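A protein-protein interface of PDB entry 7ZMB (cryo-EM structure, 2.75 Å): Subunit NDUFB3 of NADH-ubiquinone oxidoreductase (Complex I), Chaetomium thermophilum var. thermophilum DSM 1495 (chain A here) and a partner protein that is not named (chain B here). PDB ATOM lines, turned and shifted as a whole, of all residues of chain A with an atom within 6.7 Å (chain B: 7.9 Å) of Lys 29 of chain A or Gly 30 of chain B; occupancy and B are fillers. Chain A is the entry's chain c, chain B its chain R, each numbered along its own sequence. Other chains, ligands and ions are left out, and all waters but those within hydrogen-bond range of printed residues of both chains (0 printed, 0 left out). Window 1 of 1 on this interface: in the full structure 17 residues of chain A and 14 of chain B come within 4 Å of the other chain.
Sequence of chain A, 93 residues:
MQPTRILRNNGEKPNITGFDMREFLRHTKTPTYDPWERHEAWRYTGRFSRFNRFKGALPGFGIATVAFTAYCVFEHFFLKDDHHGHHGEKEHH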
ATOM      1  N   LEU A  25       1.233  22.745   5.586  1.00  0.00           N
ATOM      2  CA  LEU A  25       0.799  22.132   6.832  1.00  0.00           C
ATOM      3  C   LEU A  25       1.234  22.933   8.052  1.00  0.00           C
ATOM      4  O   LEU A  25       0.588  22.841   9.102  1.00  0.00           O
ATOM      5  CB  LEU A  25       1.338  20.703   6.917  1.00  0.00           C
ATOM      6  CG  LEU A  25       0.918  19.884   8.134  1.00  0.00           C
ATOM      7  CD1 LEU A  25      -0.589  19.709   8.113  1.00  0.00           C
ATOM      8  CD2 LEU A  25       1.624  18.539   8.155  1.00  0.00           C
ATOM      9  N   ARG A  26       2.308  23.718   7.937  1.00  0.00           N
ATOM     10  CA  ARG A  26       2.779  24.503   9.074  1.00  0.00           C
ATOM     11  C   ARG A  26       1.749  25.545   9.491  1.00  0.00           C
ATOM     12  O   ARG A  26       1.554  25.791  10.688  1.00  0.00           O
ATOM     13  CB  ARG A  26       4.111  25.170   8.739  1.00  0.00           C
ATOM     14  N   HIS A  27       1.082  26.165   8.523  1.00  0.00           N
ATOM     15  CA  HIS A  27       0.099  27.202   8.807  1.00  0.00           C
ATOM     16  C   HIS A  27      -1.239  26.644   9.282  1.00  0.00           C
ATOM     17  O   HIS A  27      -2.214  27.398   9.356  1.00  0.00           O
ATOM     18  CB  HIS A  27      -0.112  28.076   7.569  1.00  0.00           C
ATOM     19  CG  HIS A  27       0.920  29.148   7.405  1.00  0.00           C
ATOM     20  ND1 HIS A  27       0.640  30.371   6.836  1.00  0.00           N
ATOM     21  CD2 HIS A  27       2.232  29.179   7.738  1.00  0.00           C
ATOM     22  CE1 HIS A  27       1.735  31.110   6.824  1.00  0.00           C
ATOM     23  NE2 HIS A  27       2.716  30.410   7.366  1.00  0.00           N
ATOM     24  N   THR A  28      -1.310  25.353   9.606  1.00  0.00           N
ATOM     25  CA  THR A  28      -2.540  24.751  10.124  1.00  0.00           C
ATOM     26  C   THR A  28      -2.616  25.022  11.624  1.00  0.00           C
ATOM     27  O   THR A  28      -2.338  24.164  12.466  1.00  0.00           O
ATOM     28  CB  THR A  28      -2.586  23.261   9.819  1.00  0.00           C
ATOM     29  OG1 THR A  28      -1.481  22.607  10.456  1.00  0.00           O
ATOM     30  CG2 THR A  28      -2.521  23.021   8.318  1.00  0.00           C
ATOM     31  N   LYS A  29      -2.995  26.252  11.954  1.00  0.00           N
ATOM     32  CA  LYS A  29      -3.179  26.671  13.336  1.00  0.00           C
ATOM     33  C   LYS A  29      -4.005  27.947  13.335  1.00  0.00           C
ATOM     34  O   LYS A  29      -4.222  28.568  12.291  1.00  0.00           O
ATOM     35  CB  LYS A  29      -1.836  26.881  14.045  1.00  0.00           C
ATOM     36  N   THR A  30      -4.466  28.329  14.514  1.00  0.00           N
ATOM     37  CA  THR A  30      -5.216  29.571  14.647  1.00  0.00           C
ATOM     38  C   THR A  30      -4.288  30.748  14.378  1.00  0.00           C
ATOM     39  O   THR A  30      -3.259  30.880  15.054  1.00  0.00           O
ATOM     40  CB  THR A  30      -5.829  29.682  16.039  1.00  0.00           C
ATOM     41  OG1 THR A  30      -6.893  28.732  16.170  1.00  0.00           O
ATOM     42  CG2 THR A  30      -6.378  31.079  16.267  1.00  0.00           C
ATOM     43  N   PRO A  31      -4.598  31.616  13.419  1.00  0.00           N
ATOM     44  CA  PRO A  31      -3.676  32.708  13.088  1.00  0.00           C
ATOM     45  C   PRO A  31      -3.747  33.835  14.105  1.00  0.00           C
ATOM     46  O   PRO A  31      -4.815  34.161  14.629  1.00  0.00           O
ATOM     47  CB  PRO A  31      -4.152  33.175  11.706  1.00  0.00           C
ATOM     48  CG  PRO A  31      -5.540  32.620  11.534  1.00  0.00           C
ATOM     49  CD  PRO A  31      -5.866  31.708  12.679  1.00  0.00           C
ATOM     50  N   THR A  32      -2.584  34.428  14.385  1.00  0.00           N
ATOM     51  CA  THR A  32      -2.536  35.558  15.306  1.00  0.00           C
ATOM     52  C   THR A  32      -3.323  36.743  14.765  1.00  0.00           C
ATOM     53  O   THR A  32      -4.093  37.376  15.498  1.00  0.00           O
ATOM     54  CB  THR A  32      -1.085  35.955  15.573  1.00  0.00           C
ATOM     55  OG1 THR A  32      -0.463  36.357  14.346  1.00  0.00           O
ATOM     56  CG2 THR A  32      -0.316  34.785  16.166  1.00  0.00           C
ATOM     57  N   ASP A  34      -5.940  38.015  11.482  1.00  0.00           N
ATOM     58  CA  ASP A  34      -6.921  37.479  10.551  1.00  0.00           C
ATOM     59  C   ASP A  34      -8.069  38.472  10.406  1.00  0.00           C
ATOM     60  O   ASP A  34      -8.402  39.178  11.365  1.00  0.00           O
ATOM     61  CB  ASP A  34      -7.403  36.114  11.043  1.00  0.00           C
ATOM     62  CG  ASP A  34      -8.415  35.481  10.132  1.00  0.00           C
ATOM     63  OD1 ASP A  34      -8.056  35.087   9.006  1.00  0.00           O
ATOM     64  OD2 ASP A  34      -9.571  35.344  10.568  1.00  0.00           O
ATOM     65  N   HIS B  24     -12.616  20.652  11.359  1.00  0.00           N
ATOM     66  CA  HIS B  24     -12.440  21.767  12.284  1.00  0.00           C
ATOM     67  C   HIS B  24     -11.945  22.972  11.498  1.00  0.00           C
ATOM     68  O   HIS B  24     -10.770  23.036  11.125  1.00  0.00           O
ATOM     69  CB  HIS B  24     -11.459  21.396  13.390  1.00  0.00           C
ATOM     70  CG  HIS B  24     -11.805  20.129  14.104  1.00  0.00           C
ATOM     71  ND1 HIS B  24     -11.120  18.951  13.903  1.00  0.00           N
ATOM     72  CD2 HIS B  24     -12.761  19.855  15.022  1.00  0.00           C
ATOM     73  CE1 HIS B  24     -11.639  18.005  14.666  1.00  0.00           C
ATOM     74  NE2 HIS B  24     -12.638  18.528  15.355  1.00  0.00           N
ATOM     75  N   ARG B  25     -12.832  23.930  11.247  1.00  0.00           N
ATOM     76  CA  ARG B  25     -12.543  24.992  10.294  1.00  0.00           C
ATOM     77  C   ARG B  25     -11.780  26.160  10.896  1.00  0.00           C
ATOM     78  O   ARG B  25     -11.456  27.104  10.167  1.00  0.00           O
ATOM     79  CB  ARG B  25     -13.836  25.496   9.650  1.00  0.00           C
ATOM     80  CG  ARG B  25     -14.701  26.359  10.538  1.00  0.00           C
ATOM     81  CD  ARG B  25     -16.085  26.496   9.934  1.00  0.00           C
ATOM     82  NE  ARG B  25     -16.049  27.108   8.609  1.00  0.00           N
ATOM     83  CZ  ARG B  25     -16.642  28.256   8.300  1.00  0.00           C
ATOM     84  NH1 ARG B  25     -17.321  28.921   9.224  1.00  0.00           N
ATOM     85  NH2 ARG B  25     -16.557  28.740   7.070  1.00  0.00           N
ATOM     86  N   ASN B  26     -11.483  26.138  12.196  1.00  0.00           N
ATOM     87  CA  ASN B  26     -10.491  27.081  12.697  1.00  0.00           C
ATOM     88  C   ASN B  26      -9.099  26.717  12.197  1.00  0.00           C
ATOM     89  O   ASN B  26      -8.275  27.606  11.956  1.00  0.00           O
ATOM     90  CB  ASN B  26     -10.575  27.184  14.227  1.00  0.00           C
ATOM     91  CG  ASN B  26      -9.999  25.977  14.963  1.00  0.00           C
ATOM     92  OD1 ASN B  26      -9.086  25.306  14.497  1.00  0.00           O
ATOM     93  ND2 ASN B  26     -10.554  25.701  16.135  1.00  0.00           N
ATOM     94  N   LEU B  27      -8.822  25.420  12.029  1.00  0.00           N
ATOM     95  CA  LEU B  27      -7.662  25.014  11.244  1.00  0.00           C
ATOM     96  C   LEU B  27      -7.767  25.536   9.818  1.00  0.00           C
ATOM     97  O   LEU B  27      -6.791  26.051   9.261  1.00  0.00           O
ATOM     98  CB  LEU B  27      -7.525  23.490  11.229  1.00  0.00           C
ATOM     99  CG  LEU B  27      -6.825  22.708  12.348  1.00  0.00           C
ATOM    100  CD1 LEU B  27      -5.356  23.086  12.421  1.00  0.00           C
ATOM    101  CD2 LEU B  27      -7.494  22.858  13.699  1.00  0.00           C
ATOM    102  N   TRP B  28      -8.950  25.409   9.212  1.00  0.00           N
ATOM    103  CA  TRP B  28      -9.161  25.941   7.870  1.00  0.00           C
ATOM    104  C   TRP B  28      -9.071  27.459   7.850  1.00  0.00           C
ATOM    105  O   TRP B  28      -8.730  28.044   6.816  1.00  0.00           O
ATOM    106  CB  TRP B  28     -10.516  25.483   7.333  1.00  0.00           C
ATOM    107  CG  TRP B  28     -10.966  26.204   6.103  1.00  0.00           C
ATOM    108  CD1 TRP B  28     -10.609  25.932   4.821  1.00  0.00           C
ATOM    109  CD2 TRP B  28     -11.860  27.318   6.042  1.00  0.00           C
ATOM    110  NE1 TRP B  28     -11.226  26.804   3.961  1.00  0.00           N
ATOM    111  CE2 TRP B  28     -12.000  27.668   4.688  1.00  0.00           C
ATOM    112  CE3 TRP B  28     -12.557  28.056   7.003  1.00  0.00           C
ATOM    113  CZ2 TRP B  28     -12.806  28.723   4.267  1.00  0.00           C
ATOM    114  CZ3 TRP B  28     -13.357  29.102   6.585  1.00  0.00           C
ATOM    115  CH2 TRP B  28     -13.476  29.425   5.229  1.00  0.00           C
ATOM    116  N   ARG B  29      -9.371  28.109   8.975  1.00  0.00           N
ATOM    117  CA  ARG B  29      -9.361  29.566   9.006  1.00  0.00           C
ATOM    118  C   ARG B  29      -7.970  30.105   8.701  1.00  0.00           C
ATOM    119  O   ARG B  29      -7.805  30.989   7.854  1.00  0.00           O
ATOM    120  CB  ARG B  29      -9.852  30.068  10.362  1.00  0.00           C
ATOM    121  CG  ARG B  29      -9.842  31.580  10.492  1.00  0.00           C
ATOM    122  CD  ARG B  29     -10.928  32.181   9.613  1.00  0.00           C
ATOM    123  NE  ARG B  29     -10.477  32.380   8.239  1.00  0.00           N
ATOM    124  CZ  ARG B  29     -11.272  32.734   7.237  1.00  0.00           C
ATOM    125  NH1 ARG B  29     -12.568  32.911   7.449  1.00  0.00           N
ATOM    126  NH2 ARG B  29     -10.774  32.896   6.019  1.00  0.00           N
ATOM    127  N   GLY B  30      -6.953  29.572   9.377  1.00  0.00           N
ATOM    128  CA  GLY B  30      -5.585  29.915   9.036  1.00  0.00           C
ATOM    129  C   GLY B  30      -5.105  29.268   7.756  1.00  0.00           C
ATOM    130  O   GLY B  30      -4.127  29.735   7.164  1.00  0.00           O
ATOM    131  N   GLN B  31      -5.777  28.204   7.315  1.00  0.00           N
ATOM    132  CA  GLN B  31      -5.394  27.543   6.073  1.00  0.00           C
ATOM    133  C   GLN B  31      -5.592  28.466   4.879  1.00  0.00           C
ATOM    134  O   GLN B  31      -4.784  28.465   3.942  1.00  0.00           O
ATOM    135  CB  GLN B  31      -6.202  26.258   5.897  1.00  0.00           C
ATOM    136  CG  GLN B  31      -5.821  25.465   4.672  1.00  0.00           C
ATOM    137  CD  GLN B  31      -4.389  24.998   4.729  1.00  0.00           C
ATOM    138  OE1 GLN B  31      -3.521  25.544   4.054  1.00  0.00           O
ATOM    139  NE2 GLN B  31      -4.134  23.971   5.530  1.00  0.00           N
ATOM    140  N   ALA B  32      -6.664  29.259   4.892  1.00  0.00           N
ATOM    141  CA  ALA B  32      -6.947  30.148   3.770  1.00  0.00           C
ATOM    142  C   ALA B  32      -5.892  31.235   3.627  1.00  0.00           C
ATOM    143  O   ALA B  32      -5.595  31.661   2.505  1.00  0.00           O
ATOM    144  CB  ALA B  32      -8.331  30.776   3.932  1.00  0.00           C
ATOM    145  N   LEU B  33      -5.319  31.696   4.741  1.00  0.00           N
ATOM    146  CA  LEU B  33      -4.318  32.756   4.672  1.00  0.00           C
ATOM    147  C   LEU B  33      -3.097  32.303   3.886  1.00  0.00           C
ATOM    148  O   LEU B  33      -2.542  33.070   3.089  1.00  0.00           O
ATOM    149  CB  LEU B  33      -3.919  33.203   6.077  1.00  0.00           C
ATOM    150  CG  LEU B  33      -4.826  34.224   6.770  1.00  0.00           C
ATOM    151  CD1 LEU B  33      -4.824  35.537   6.005  1.00  0.00           C
ATOM    152  CD2 LEU B  33      -6.241  33.700   6.931  1.00  0.00           C
ATOM    153  N   TYR B  34      -2.658  31.061   4.099  1.00  0.00           N
ATOM    154  CA  TYR B  34      -1.607  30.503   3.259  1.00  0.00           C
ATOM    155  C   TYR B  34      -2.054  30.437   1.806  1.00  0.00           C
ATOM    156  O   TYR B  34      -1.281  30.752   0.895  1.00  0.00           O
ATOM    157  CB  TYR B  34      -1.212  29.115   3.760  1.00  0.00           C
ATOM    158  CG  TYR B  34      -0.099  28.481   2.962  1.00  0.00           C
ATOM    159  CD1 TYR B  34       1.216  28.893   3.121  1.00  0.00           C
ATOM    160  CD2 TYR B  34      -0.363  27.476   2.044  1.00  0.00           C
ATOM    161  CE1 TYR B  34       2.236  28.317   2.392  1.00  0.00           C
ATOM    162  CE2 TYR B  34       0.649  26.894   1.310  1.00  0.00           C
ATOM    163  CZ  TYR B  34       1.948  27.318   1.488  1.00  0.00           C
ATOM    164  OH  TYR B  34       2.959  26.739   0.757  1.00  0.00           O
ATOM    165  N   ILE B  35      -3.301  30.027   1.573  1.00  0.00           N
ATOM    166  CA  ILE B  35      -3.847  30.050   0.221  1.00  0.00           C
ATOM    167  C   ILE B  35      -3.963  31.482  -0.279  1.00  0.00           C
ATOM    168  O   ILE B  35      -3.639  31.778  -1.436  1.00  0.00           O
ATOM    169  CB  ILE B  35      -5.203  29.323   0.183  1.00  0.00           C
ATOM    170  CG1 ILE B  35      -5.044  27.874   0.648  1.00  0.00           C
ATOM    171  CG2 ILE B  35      -5.792  29.367  -1.216  1.00  0.00           C
ATOM    172  CD1 ILE B  35      -4.154  27.040  -0.244  1.00  0.00           C
ATOM    173  N   ARG B  36      -4.424  32.395   0.580  1.00  0.00           N
ATOM    174  CA  ARG B  36      -4.576  33.788   0.172  1.00  0.00           C
ATOM    175  C   ARG B  36      -3.235  34.407  -0.197  1.00  0.00           C
ATOM    176  O   ARG B  36      -3.084  34.992  -1.276  1.00  0.00           O
ATOM    177  CB  ARG B  36      -5.229  34.600   1.288  1.00  0.00           C
ATOM    178  CG  ARG B  36      -5.486  36.027   0.874  1.00  0.00           C
ATOM    179  CD  ARG B  36      -6.212  36.828   1.929  1.00  0.00           C
ATOM    180  NE  ARG B  36      -6.343  38.207   1.482  1.00  0.00           N
ATOM    181  CZ  ARG B  36      -7.342  38.644   0.728  1.00  0.00           C
ATOM    182  NH1 ARG B  36      -7.389  39.911   0.342  1.00  0.00           N
ATOM    183  NH2 ARG B  36      -8.314  37.815   0.377  1.00  0.00           N
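Along chain A the printed residues that touch a printed residue of chain B span positions 27 to 34.
O of Leu 25 of chain A is in hydrogen-bond range of OG1 of Thr 28 of chain A.
Among the printed residues, merely in contact across the chains: Asp 34 of chain A with Leu 33 of chain B, Thr 28 of chain A with Leu 27 of chain B, Thr 28 of chain A with Gln 31 of chain B, Pro 31 of chain A with Gly 30 of chain B, His 27 of chain A with Gly 30 of chain B, Lys 29 of chain A with Gly 30 of chain B, His 27 of chain A with Tyr 34 of chain B and Lys 29 of chain A with Leu 27 of chain B.
The guanidinium group of Arg 29 of chain B lies within salt-bridge range of the side-chain carboxylate of Asp 34 of chain A (3.7 Å).
Lys 29 of chain A touches just these residues of chain B: Leu 27 and Gly 30. Of the printed residues of chain B, Asp 34 of chain A touches Arg 29 and Leu 33. Arg 25 of chain B touches none of the printed residues of chain A. Of the printed residues of chain A, Arg 29 of chain B touches Asp 34. Gly 30 of chain B touches three residues of chain A. Printed residues of chain A within 4 Å of Gln 31 of chain B: Thr 28 (3.4 Å). The nearest residue of chain B that does not touch Lys 29 of chain A is Asn 26 of chain B (4.2 Å). The nearest residue of chain A that does not touch Gly 30 of chain B is Thr 30 of chain A (5.5 Å).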
